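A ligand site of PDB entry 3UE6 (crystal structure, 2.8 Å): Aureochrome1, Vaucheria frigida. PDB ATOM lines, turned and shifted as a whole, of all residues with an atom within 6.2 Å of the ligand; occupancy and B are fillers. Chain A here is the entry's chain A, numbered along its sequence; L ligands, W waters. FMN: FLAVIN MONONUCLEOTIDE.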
ATOM      1  N   VAL A  49     -13.895 -23.528 -26.799  1.00  0.00           N
ATOM      2  CA  VAL A  49     -15.015 -23.327 -27.709  1.00  0.00           C
ATOM      3  C   VAL A  49     -15.972 -22.273 -27.159  1.00  0.00           C
ATOM      4  O   VAL A  49     -15.919 -21.927 -25.974  1.00  0.00           O
ATOM      5  CB  VAL A  49     -15.789 -24.645 -27.958  1.00  0.00           C
ATOM      6  CG1 VAL A  49     -14.880 -25.709 -28.563  1.00  0.00           C
ATOM      7  CG2 VAL A  49     -16.395 -25.142 -26.658  1.00  0.00           C
ATOM      8  N   ILE A  50     -16.817 -21.746 -28.030  1.00  0.00           N
ATOM      9  CA  ILE A  50     -17.899 -20.859 -27.621  1.00  0.00           C
ATOM     10  C   ILE A  50     -19.217 -21.434 -28.134  1.00  0.00           C
ATOM     11  O   ILE A  50     -19.341 -21.752 -29.313  1.00  0.00           O
ATOM     12  CB  ILE A  50     -17.748 -19.455 -28.220  1.00  0.00           C
ATOM     13  CG1 ILE A  50     -16.340 -18.899 -28.002  1.00  0.00           C
ATOM     14  CG2 ILE A  50     -18.795 -18.514 -27.618  1.00  0.00           C
ATOM     15  CD1 ILE A  50     -16.118 -18.346 -26.610  1.00  0.00           C
ATOM     16  N   THR A  51     -20.193 -21.567 -27.241  1.00  0.00           N
ATOM     17  CA  THR A  51     -21.515 -22.021 -27.650  1.00  0.00           C
ATOM     18  C   THR A  51     -22.532 -20.895 -27.555  1.00  0.00           C
ATOM     19  O   THR A  51     -22.327 -19.928 -26.814  1.00  0.00           O
ATOM     20  CB  THR A  51     -21.990 -23.199 -26.778  1.00  0.00           C
ATOM     21  OG1 THR A  51     -22.216 -22.742 -25.445  1.00  0.00           O
ATOM     22  CG2 THR A  51     -20.950 -24.303 -26.776  1.00  0.00           C
ATOM     23  N   ASP A  57     -30.288 -26.280 -28.331  1.00  0.00           N
ATOM     24  CA  ASP A  57     -29.322 -27.299 -27.892  1.00  0.00           C
ATOM     25  C   ASP A  57     -27.873 -26.800 -27.773  1.00  0.00           C
ATOM     26  O   ASP A  57     -26.932 -27.570 -27.913  1.00  0.00           O
ATOM     27  CB  ASP A  57     -29.403 -28.533 -28.804  1.00  0.00           C
ATOM     28  CG  ASP A  57     -28.788 -29.767 -28.161  1.00  0.00           C
ATOM     29  OD1 ASP A  57     -28.798 -29.885 -26.916  1.00  0.00           O
ATOM     30  OD2 ASP A  57     -28.307 -30.634 -28.923  1.00  0.00           O
ATOM     31  N   ASN A  58     -27.712 -25.503 -27.516  1.00  0.00           N
ATOM     32  CA  ASN A  58     -26.402 -24.952 -27.144  1.00  0.00           C
ATOM     33  C   ASN A  58     -25.265 -25.363 -28.076  1.00  0.00           C
ATOM     34  O   ASN A  58     -24.305 -26.005 -27.647  1.00  0.00           O
ATOM     35  CB  ASN A  58     -26.085 -25.385 -25.709  1.00  0.00           C
ATOM     36  CG  ASN A  58     -25.156 -24.426 -24.993  1.00  0.00           C
ATOM     37  OD1 ASN A  58     -24.603 -24.754 -23.943  1.00  0.00           O
ATOM     38  ND2 ASN A  58     -24.998 -23.219 -25.542  1.00  0.00           N
ATOM     39  N   PHE A  67      -8.233 -26.572 -30.147  1.00  0.00           N
ATOM     40  CA  PHE A  67      -9.303 -27.530 -29.961  1.00  0.00           C
ATOM     41  C   PHE A  67      -9.446 -28.471 -31.161  1.00  0.00           C
ATOM     42  O   PHE A  67      -9.662 -29.657 -31.007  1.00  0.00           O
ATOM     43  CB  PHE A  67     -10.615 -26.802 -29.716  1.00  0.00           C
ATOM     44  CG  PHE A  67     -11.792 -27.722 -29.600  1.00  0.00           C
ATOM     45  CD1 PHE A  67     -12.208 -28.191 -28.369  1.00  0.00           C
ATOM     46  CD2 PHE A  67     -12.492 -28.120 -30.736  1.00  0.00           C
ATOM     47  CE1 PHE A  67     -13.295 -29.043 -28.258  1.00  0.00           C
ATOM     48  CE2 PHE A  67     -13.572 -28.966 -30.630  1.00  0.00           C
ATOM     49  CZ  PHE A  67     -13.975 -29.430 -29.397  1.00  0.00           C
ATOM     50  N   ASN A  82     -23.642 -29.797 -30.664  1.00  0.00           N
ATOM     51  CA  ASN A  82     -23.400 -29.833 -29.223  1.00  0.00           C
ATOM     52  C   ASN A  82     -22.127 -30.636 -28.901  1.00  0.00           C
ATOM     53  O   ASN A  82     -21.835 -31.633 -29.575  1.00  0.00           O
ATOM     54  CB  ASN A  82     -24.614 -30.433 -28.497  1.00  0.00           C
ATOM     55  CG  ASN A  82     -24.459 -30.425 -26.988  1.00  0.00           C
ATOM     56  OD1 ASN A  82     -23.801 -31.291 -26.406  1.00  0.00           O
ATOM     57  ND2 ASN A  82     -25.076 -29.442 -26.336  1.00  0.00           N
ATOM     58  N   CYS A  83     -21.396 -30.214 -27.877  1.00  0.00           N
ATOM     59  CA  CYS A  83     -20.079 -30.781 -27.575  1.00  0.00           C
ATOM     60  C   CYS A  83     -20.108 -32.235 -27.125  1.00  0.00           C
ATOM     61  O   CYS A  83     -19.067 -32.852 -26.930  1.00  0.00           O
ATOM     62  CB  CYS A  83     -19.367 -29.944 -26.512  1.00  0.00           C
ATOM     63  SG  CYS A  83     -18.969 -28.268 -27.010  1.00  0.00           S
ATOM     64  N   ARG A  84     -21.304 -32.791 -26.953  1.00  0.00           N
ATOM     65  CA  ARG A  84     -21.424 -34.142 -26.431  1.00  0.00           C
ATOM     66  C   ARG A  84     -20.819 -35.174 -27.382  1.00  0.00           C
ATOM     67  O   ARG A  84     -20.655 -36.333 -27.016  1.00  0.00           O
ATOM     68  CB  ARG A  84     -22.881 -34.497 -26.138  1.00  0.00           C
ATOM     69  CG  ARG A  84     -23.723 -34.691 -27.387  1.00  0.00           C
ATOM     70  CD  ARG A  84     -25.116 -35.176 -27.030  1.00  0.00           C
ATOM     71  NE  ARG A  84     -25.799 -34.242 -26.137  1.00  0.00           N
ATOM     72  CZ  ARG A  84     -26.543 -33.218 -26.552  1.00  0.00           C
ATOM     73  NH1 ARG A  84     -26.693 -32.987 -27.841  1.00  0.00           N
ATOM     74  NH2 ARG A  84     -27.124 -32.420 -25.677  1.00  0.00           N
ATOM     75  N   LEU A  86     -17.941 -35.491 -28.161  1.00  0.00           N
ATOM     76  CA  LEU A  86     -16.614 -35.840 -27.678  1.00  0.00           C
ATOM     77  C   LEU A  86     -16.681 -37.036 -26.758  1.00  0.00           C
ATOM     78  O   LEU A  86     -15.656 -37.618 -26.396  1.00  0.00           O
ATOM     79  CB  LEU A  86     -15.981 -34.655 -26.959  1.00  0.00           C
ATOM     80  CG  LEU A  86     -15.678 -33.443 -27.824  1.00  0.00           C
ATOM     81  CD1 LEU A  86     -15.196 -32.281 -26.959  1.00  0.00           C
ATOM     82  CD2 LEU A  86     -14.647 -33.793 -28.878  1.00  0.00           C
ATOM     83  N   GLN A  87     -17.891 -37.407 -26.373  1.00  0.00           N
ATOM     84  CA  GLN A  87     -18.099 -38.531 -25.482  1.00  0.00           C
ATOM     85  C   GLN A  87     -18.282 -39.834 -26.263  1.00  0.00           C
ATOM     86  O   GLN A  87     -18.748 -39.832 -27.401  1.00  0.00           O
ATOM     87  CB  GLN A  87     -19.321 -38.297 -24.591  1.00  0.00           C
ATOM     88  CG  GLN A  87     -19.194 -37.079 -23.701  1.00  0.00           C
ATOM     89  CD  GLN A  87     -20.538 -36.552 -23.254  1.00  0.00           C
ATOM     90  OE1 GLN A  87     -21.572 -37.214 -23.411  1.00  0.00           O
ATOM     91  NE2 GLN A  87     -20.546 -35.343 -22.689  1.00  0.00           N
ATOM     92  N   THR A  91     -17.148 -43.209 -21.458  1.00  0.00           N
ATOM     93  CA  THR A  91     -17.321 -42.001 -20.657  1.00  0.00           C
ATOM     94  C   THR A  91     -18.214 -42.237 -19.440  1.00  0.00           C
ATOM     95  O   THR A  91     -19.246 -42.907 -19.544  1.00  0.00           O
ATOM     96  CB  THR A  91     -17.866 -40.849 -21.515  1.00  0.00           C
ATOM     97  OG1 THR A  91     -17.133 -40.761 -22.733  1.00  0.00           O
ATOM     98  CG2 THR A  91     -17.779 -39.519 -20.762  1.00  0.00           C
ATOM     99  N   VAL A  96     -20.788 -36.914 -16.760  1.00  0.00           N
ATOM    100  CA  VAL A  96     -21.656 -36.186 -17.677  1.00  0.00           C
ATOM    101  C   VAL A  96     -22.844 -35.595 -16.913  1.00  0.00           C
ATOM    102  O   VAL A  96     -23.263 -34.467 -17.173  1.00  0.00           O
ATOM    103  CB  VAL A  96     -22.183 -37.066 -18.821  1.00  0.00           C
ATOM    104  CG1 VAL A  96     -23.171 -36.300 -19.682  1.00  0.00           C
ATOM    105  CG2 VAL A  96     -21.038 -37.588 -19.657  1.00  0.00           C
ATOM    106  N   ILE A  99     -21.862 -32.342 -15.336  1.00  0.00           N
ATOM    107  CA  ILE A  99     -21.812 -31.263 -16.322  1.00  0.00           C
ATOM    108  C   ILE A  99     -23.196 -30.774 -16.746  1.00  0.00           C
ATOM    109  O   ILE A  99     -23.445 -29.568 -16.815  1.00  0.00           O
ATOM    110  CB  ILE A  99     -21.011 -31.650 -17.570  1.00  0.00           C
ATOM    111  CG1 ILE A  99     -19.562 -31.971 -17.202  1.00  0.00           C
ATOM    112  CG2 ILE A  99     -21.068 -30.528 -18.597  1.00  0.00           C
ATOM    113  CD1 ILE A  99     -18.736 -32.553 -18.334  1.00  0.00           C
ATOM    114  N   ARG A 100     -24.095 -31.698 -17.054  1.00  0.00           N
ATOM    115  CA  ARG A 100     -25.455 -31.316 -17.397  1.00  0.00           C
ATOM    116  C   ARG A 100     -26.064 -30.489 -16.257  1.00  0.00           C
ATOM    117  O   ARG A 100     -26.554 -29.390 -16.481  1.00  0.00           O
ATOM    118  CB  ARG A 100     -26.312 -32.559 -17.660  1.00  0.00           C
ATOM    119  CG  ARG A 100     -27.727 -32.272 -18.127  1.00  0.00           C
ATOM    120  CD  ARG A 100     -28.376 -33.514 -18.714  1.00  0.00           C
ATOM    121  NE  ARG A 100     -28.335 -34.653 -17.789  1.00  0.00           N
ATOM    122  CZ  ARG A 100     -27.549 -35.710 -17.910  1.00  0.00           C
ATOM    123  NH1 ARG A 100     -26.718 -35.819 -18.941  1.00  0.00           N
ATOM    124  NH2 ARG A 100     -27.594 -36.680 -17.007  1.00  0.00           N
ATOM    125  N   ILE A 103     -24.726 -27.002 -15.789  1.00  0.00           N
ATOM    126  CA  ILE A 103     -25.217 -26.138 -16.853  1.00  0.00           C
ATOM    127  C   ILE A 103     -26.659 -25.672 -16.607  1.00  0.00           C
ATOM    128  O   ILE A 103     -26.967 -24.496 -16.768  1.00  0.00           O
ATOM    129  CB  ILE A 103     -25.103 -26.824 -18.225  1.00  0.00           C
ATOM    130  CG1 ILE A 103     -23.642 -26.805 -18.683  1.00  0.00           C
ATOM    131  CG2 ILE A 103     -25.996 -26.154 -19.244  1.00  0.00           C
ATOM    132  CD1 ILE A 103     -23.408 -27.458 -20.024  1.00  0.00           C
ATOM    133  N   LEU A 113     -13.199 -36.182 -17.457  1.00  0.00           N
ATOM    134  CA  LEU A 113     -13.827 -37.370 -18.052  1.00  0.00           C
ATOM    135  C   LEU A 113     -13.099 -37.851 -19.306  1.00  0.00           C
ATOM    136  O   LEU A 113     -12.338 -37.096 -19.929  1.00  0.00           O
ATOM    137  CB  LEU A 113     -15.308 -37.109 -18.372  1.00  0.00           C
ATOM    138  CG  LEU A 113     -15.782 -35.774 -18.976  1.00  0.00           C
ATOM    139  CD1 LEU A 113     -14.780 -35.169 -19.946  1.00  0.00           C
ATOM    140  CD2 LEU A 113     -17.131 -35.957 -19.656  1.00  0.00           C
ATOM    141  N   LEU A 114     -13.325 -39.111 -19.661  1.00  0.00           N
ATOM    142  CA  LEU A 114     -12.766 -39.688 -20.882  1.00  0.00           C
ATOM    143  C   LEU A 114     -13.488 -39.134 -22.113  1.00  0.00           C
ATOM    144  O   LEU A 114     -14.702 -39.276 -22.246  1.00  0.00           O
ATOM    145  CB  LEU A 114     -12.910 -41.203 -20.859  1.00  0.00           C
ATOM    146  CG  LEU A 114     -12.032 -41.957 -21.852  1.00  0.00           C
ATOM    147  CD1 LEU A 114     -10.573 -41.717 -21.512  1.00  0.00           C
ATOM    148  CD2 LEU A 114     -12.355 -43.451 -21.846  1.00  0.00           C
ATOM    149  N   ASN A 115     -12.721 -38.519 -23.003  1.00  0.00           N
ATOM    150  CA  ASN A 115     -13.254 -38.052 -24.286  1.00  0.00           C
ATOM    151  C   ASN A 115     -12.628 -38.774 -25.476  1.00  0.00           C
ATOM    152  O   ASN A 115     -11.596 -39.424 -25.352  1.00  0.00           O
ATOM    153  CB  ASN A 115     -13.081 -36.540 -24.438  1.00  0.00           C
ATOM    154  CG  ASN A 115     -14.142 -35.743 -23.726  1.00  0.00           C
ATOM    155  OD1 ASN A 115     -14.080 -34.509 -23.671  1.00  0.00           O
ATOM    156  ND2 ASN A 115     -15.127 -36.437 -23.150  1.00  0.00           N
ATOM    157  N   ASN A 125      -9.974 -35.706 -20.113  1.00  0.00           N
ATOM    158  CA  ASN A 125     -10.190 -34.273 -20.308  1.00  0.00           C
ATOM    159  C   ASN A 125     -10.609 -33.552 -19.038  1.00  0.00           C
ATOM    160  O   ASN A 125     -11.715 -33.744 -18.545  1.00  0.00           O
ATOM    161  CB  ASN A 125     -11.259 -34.071 -21.398  1.00  0.00           C
ATOM    162  CG  ASN A 125     -11.487 -32.612 -21.719  1.00  0.00           C
ATOM    163  OD1 ASN A 125     -10.761 -31.736 -21.262  1.00  0.00           O
ATOM    164  ND2 ASN A 125     -12.509 -32.346 -22.527  1.00  0.00           N
ATOM    165  N   PHE A 127     -12.052 -30.521 -17.990  1.00  0.00           N
ATOM    166  CA  PHE A 127     -12.820 -29.621 -18.811  1.00  0.00           C
ATOM    167  C   PHE A 127     -13.573 -28.608 -17.930  1.00  0.00           C
ATOM    168  O   PHE A 127     -14.271 -28.978 -16.996  1.00  0.00           O
ATOM    169  CB  PHE A 127     -13.743 -30.455 -19.691  1.00  0.00           C
ATOM    170  CG  PHE A 127     -15.082 -29.849 -19.934  1.00  0.00           C
ATOM    171  CD1 PHE A 127     -15.204 -28.753 -20.771  1.00  0.00           C
ATOM    172  CD2 PHE A 127     -16.210 -30.392 -19.353  1.00  0.00           C
ATOM    173  CE1 PHE A 127     -16.444 -28.196 -21.009  1.00  0.00           C
ATOM    174  CE2 PHE A 127     -17.447 -29.842 -19.596  1.00  0.00           C
ATOM    175  CZ  PHE A 127     -17.565 -28.741 -20.422  1.00  0.00           C
ATOM    176  N   PHE A 128     -13.392 -27.318 -18.225  1.00  0.00           N
ATOM    177  CA  PHE A 128     -14.060 -26.247 -17.489  1.00  0.00           C
ATOM    178  C   PHE A 128     -15.092 -25.545 -18.362  1.00  0.00           C
ATOM    179  O   PHE A 128     -14.883 -25.345 -19.558  1.00  0.00           O
ATOM    180  CB  PHE A 128     -13.055 -25.234 -16.937  1.00  0.00           C
ATOM    181  CG  PHE A 128     -13.698 -24.023 -16.280  1.00  0.00           C
ATOM    182  CD1 PHE A 128     -14.122 -24.066 -14.961  1.00  0.00           C
ATOM    183  CD2 PHE A 128     -13.835 -22.833 -16.981  1.00  0.00           C
ATOM    184  CE1 PHE A 128     -14.702 -22.945 -14.358  1.00  0.00           C
ATOM    185  CE2 PHE A 128     -14.413 -21.720 -16.383  1.00  0.00           C
ATOM    186  CZ  PHE A 128     -14.843 -21.784 -15.077  1.00  0.00           C
ATOM    187  N   VAL A 129     -16.219 -25.172 -17.750  1.00  0.00           N
ATOM    188  CA  VAL A 129     -17.288 -24.481 -18.459  1.00  0.00           C
ATOM    189  C   VAL A 129     -17.798 -23.277 -17.664  1.00  0.00           C
ATOM    190  O   VAL A 129     -17.911 -23.331 -16.430  1.00  0.00           O
ATOM    191  CB  VAL A 129     -18.457 -25.443 -18.792  1.00  0.00           C
ATOM    192  CG1 VAL A 129     -18.977 -26.130 -17.534  1.00  0.00           C
ATOM    193  CG2 VAL A 129     -19.581 -24.705 -19.492  1.00  0.00           C
ATOM    194  N   ALA A 130     -18.082 -22.173 -18.352  1.00  0.00           N
ATOM    195  CA  ALA A 130     -18.585 -20.968 -17.708  1.00  0.00           C
ATOM    196  C   ALA A 130     -19.645 -20.268 -18.539  1.00  0.00           C
ATOM    197  O   ALA A 130     -19.458 -20.028 -19.733  1.00  0.00           O
ATOM    198  CB  ALA A 130     -17.434 -20.001 -17.413  1.00  0.00           C
ATOM    199  N   TYR A 142     -21.722 -19.741 -23.679  1.00  0.00           N
ATOM    200  CA  TYR A 142     -20.873 -20.543 -22.817  1.00  0.00           C
ATOM    201  C   TYR A 142     -19.470 -20.603 -23.406  1.00  0.00           C
ATOM    202  O   TYR A 142     -19.304 -20.625 -24.625  1.00  0.00           O
ATOM    203  CB  TYR A 142     -21.431 -21.963 -22.674  1.00  0.00           C
ATOM    204  CG  TYR A 142     -22.567 -22.117 -21.684  1.00  0.00           C
ATOM    205  CD1 TYR A 142     -22.310 -22.356 -20.331  1.00  0.00           C
ATOM    206  CD2 TYR A 142     -23.887 -22.044 -22.093  1.00  0.00           C
ATOM    207  CE1 TYR A 142     -23.346 -22.499 -19.424  1.00  0.00           C
ATOM    208  CE2 TYR A 142     -24.932 -22.200 -21.193  1.00  0.00           C
ATOM    209  CZ  TYR A 142     -24.657 -22.421 -19.855  1.00  0.00           C
ATOM    210  OH  TYR A 142     -25.682 -22.573 -18.946  1.00  0.00           O
ATOM    211  N   VAL A 143     -18.463 -20.608 -22.539  1.00  0.00           N
ATOM    212  CA  VAL A 143     -17.107 -20.864 -22.982  1.00  0.00           C
ATOM    213  C   VAL A 143     -16.614 -22.174 -22.363  1.00  0.00           C
ATOM    214  O   VAL A 143     -16.665 -22.355 -21.148  1.00  0.00           O
ATOM    215  CB  VAL A 143     -16.151 -19.686 -22.632  1.00  0.00           C
ATOM    216  CG1 VAL A 143     -16.265 -19.312 -21.157  1.00  0.00           C
ATOM    217  CG2 VAL A 143     -14.722 -20.030 -23.009  1.00  0.00           C
ATOM    218  N   GLY A 144     -16.187 -23.108 -23.215  1.00  0.00           N
ATOM    219  CA  GLY A 144     -15.661 -24.377 -22.750  1.00  0.00           C
ATOM    220  C   GLY A 144     -14.166 -24.437 -22.915  1.00  0.00           C
ATOM    221  O   GLY A 144     -13.630 -24.010 -23.945  1.00  0.00           O
ATOM    222  N   VAL A 145     -13.470 -24.966 -21.910  1.00  0.00           N
ATOM    223  CA  VAL A 145     -12.022 -25.090 -21.971  1.00  0.00           C
ATOM    224  C   VAL A 145     -11.591 -26.537 -21.765  1.00  0.00           C
ATOM    225  O   VAL A 145     -11.869 -27.131 -20.715  1.00  0.00           O
ATOM    226  CB  VAL A 145     -11.322 -24.199 -20.940  1.00  0.00           C
ATOM    227  CG1 VAL A 145      -9.816 -24.407 -20.991  1.00  0.00           C
ATOM    228  CG2 VAL A 145     -11.670 -22.739 -21.169  1.00  0.00           C
ATOM    229  N   GLN A 146     -10.920 -27.106 -22.751  1.00  0.00           N
ATOM    230  CA  GLN A 146     -10.468 -28.489 -22.682  1.00  0.00           C
ATOM    231  C   GLN A 146      -8.963 -28.566 -22.431  1.00  0.00           C
ATOM    232  O   GLN A 146      -8.219 -27.663 -22.790  1.00  0.00           O
ATOM    233  CB  GLN A 146     -10.822 -29.235 -23.970  1.00  0.00           C
ATOM    234  CG  GLN A 146     -12.310 -29.297 -24.270  1.00  0.00           C
ATOM    235  CD  GLN A 146     -12.875 -27.976 -24.742  1.00  0.00           C
ATOM    236  OE1 GLN A 146     -12.130 -27.106 -25.223  1.00  0.00           O
ATOM    237  NE2 GLN A 146     -14.185 -27.802 -24.607  1.00  0.00           N
HETATM  238  N1  FMN L   1     -18.720 -32.426 -22.752  1.00  0.00           N
HETATM  239  C2  FMN L   1     -17.632 -33.255 -22.939  1.00  0.00           C
HETATM  240  O2  FMN L   1     -17.736 -34.465 -22.732  1.00  0.00           O
HETATM  241  N3  FMN L   1     -16.434 -32.722 -23.362  1.00  0.00           N
HETATM  242  C4  FMN L   1     -16.311 -31.370 -23.614  1.00  0.00           C
HETATM  243  O4  FMN L   1     -15.249 -30.905 -23.989  1.00  0.00           O
HETATM  244  C4A FMN L   1     -17.416 -30.539 -23.425  1.00  0.00           C
HETATM  245  N5  FMN L   1     -17.313 -29.177 -23.668  1.00  0.00           N
HETATM  246  C5A FMN L   1     -18.414 -28.361 -23.472  1.00  0.00           C
HETATM  247  C6  FMN L   1     -18.298 -26.994 -23.713  1.00  0.00           C
HETATM  248  C7  FMN L   1     -19.397 -26.156 -23.528  1.00  0.00           C
HETATM  249  C7M FMN L   1     -19.269 -24.683 -23.787  1.00  0.00           C
HETATM  250  C8  FMN L   1     -20.601 -26.695 -23.100  1.00  0.00           C
HETATM  251  C8M FMN L   1     -21.778 -25.792 -22.893  1.00  0.00           C
HETATM  252  C9  FMN L   1     -20.710 -28.064 -22.851  1.00  0.00           C
HETATM  253  C9A FMN L   1     -19.611 -28.901 -23.036  1.00  0.00           C
HETATM  254  N10 FMN L   1     -19.705 -30.258 -22.815  1.00  0.00           N
HETATM  255  C10 FMN L   1     -18.614 -31.072 -23.001  1.00  0.00           C
HETATM  256  C1' FMN L   1     -20.977 -30.892 -22.326  1.00  0.00           C
HETATM  257  C2' FMN L   1     -21.952 -31.293 -23.429  1.00  0.00           C
HETATM  258  O2' FMN L   1     -22.029 -30.290 -24.405  1.00  0.00           O
HETATM  259  C3' FMN L   1     -23.322 -31.529 -22.797  1.00  0.00           C
HETATM  260  O3' FMN L   1     -23.784 -30.346 -22.169  1.00  0.00           O
HETATM  261  C4' FMN L   1     -23.228 -32.652 -21.764  1.00  0.00           C
HETATM  262  O4' FMN L   1     -22.864 -33.844 -22.424  1.00  0.00           O
HETATM  263  C5' FMN L   1     -24.540 -32.887 -21.017  1.00  0.00           C
HETATM  264  O5' FMN L   1     -25.630 -32.743 -21.899  1.00  0.00           O
HETATM  265  P   FMN L   1     -26.427 -34.021 -22.474  1.00  0.00           P
HETATM  266  O1P FMN L   1     -25.466 -34.809 -23.342  1.00  0.00           O
HETATM  267  O2P FMN L   1     -27.589 -33.567 -23.329  1.00  0.00           O
HETATM  268  O3P FMN L   1     -26.941 -34.900 -21.365  1.00  0.00           O
HETATM  269  O   HOH W   1     -24.668 -28.042 -23.422  1.00  0.00           O
HETATM  270  O   HOH W   2     -29.382 -36.224 -23.902  1.00  0.00           O
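N of Val 143 sits at hydrogen-bond distance from O of Ala 130 (3.0 Å).
OD2 of Asp 57 is in salt-bridge range of NH1 of Arg 84, 3.1 Å away.
ND2 of Asn 58 sits at hydrogen-bond distance from OG1 of Thr 51.
The side-chain amide nitrogen of Asn 115 sits close to the backbone carbonyl oxygen of Leu 86, at 3.5 Å.
O of Gly 144 is in hydrogen-bond range of N of Val 49.
ND2 of Asn 125 lies within hydrogen-bond range of OD1 of Asn 115, at 2.9 Å.
OH of Tyr 142 sits at hydrogen-bond distance from O of Ile 103 (3.2 Å).
The side-chain amide oxygen (OD1) of Asn 82 lies within hydrogen-bond range of the backbone NH (N) of Arg 84.
Water W1 lies within hydrogen-bond range of an oxygen (O3') of the ligand (2.8 Å), the side-chain amide nitrogen (ND2) of Asn 82 (3.3 Å) and the side-chain amide oxygen (OD1) of Asn 58 (3.3 Å).
The guanidinium group of Arg 100 lies within salt-bridge range of an oxygen (O3P) of the ligand, at 2.6 Å.
O4 of the ligand sits at hydrogen-bond distance from NE2 of Gln 146, at 3.3 Å.
The side-chain amide nitrogen (NE2) of Gln 87 lies within hydrogen-bond range of an oxygen (O4') of the ligand, at 2.8 Å.
An oxygen (O2P) of the ligand is in salt-bridge range of the guanidinium group of Arg 84, at 2.7 Å.
N3 of the ligand sits at hydrogen-bond distance from OD1 of Asn 115 (3.0 Å).
ND2 of Asn 125 sits at hydrogen-bond distance from O4 of the ligand, at 3.4 Å.
OD1 of Asn 82 lies within hydrogen-bond range of O2' of the ligand (2.9 Å).
CG2 of Val 49 touches C6 of the ligand (3.97 Å).
Thr 51 touches the ligand.
Asn 58 touches the ligand (OD1 to C8M, 3.2 Å).
CB of Cys 83 touches O2' of the ligand, at 3.4 Å.
Leu 86 touches the ligand (CD1 to O4, 3.3 Å).
Val 96 touches the ligand (CG1 to O4', 3.7 Å).
Ile 99 touches the ligand (CG2 to C1', 3.7 Å).
Ile 103 touches the ligand (CD1 to O3', 3.6 Å).
Leu 113 touches the ligand (CD2 to O2, 3.5 Å).
Phe 127 touches the ligand.
Tyr 142 touches the ligand.
Val 143 touches the ligand.
N of Gly 144 touches C7M of the ligand, 3.5 Å away.
20 residues have an atom within 4 Å of the ligand: Val 49, Thr 51, Asn 58, Asn 82, Cys 83, Arg 84, Leu 86, Gln 87, Val 96, Ile 99, Arg 100, Ile 103, Leu 113, Asn 115, Asn 125, Phe 127, Tyr 142, Val 143, Gly 144 and Gln 146.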
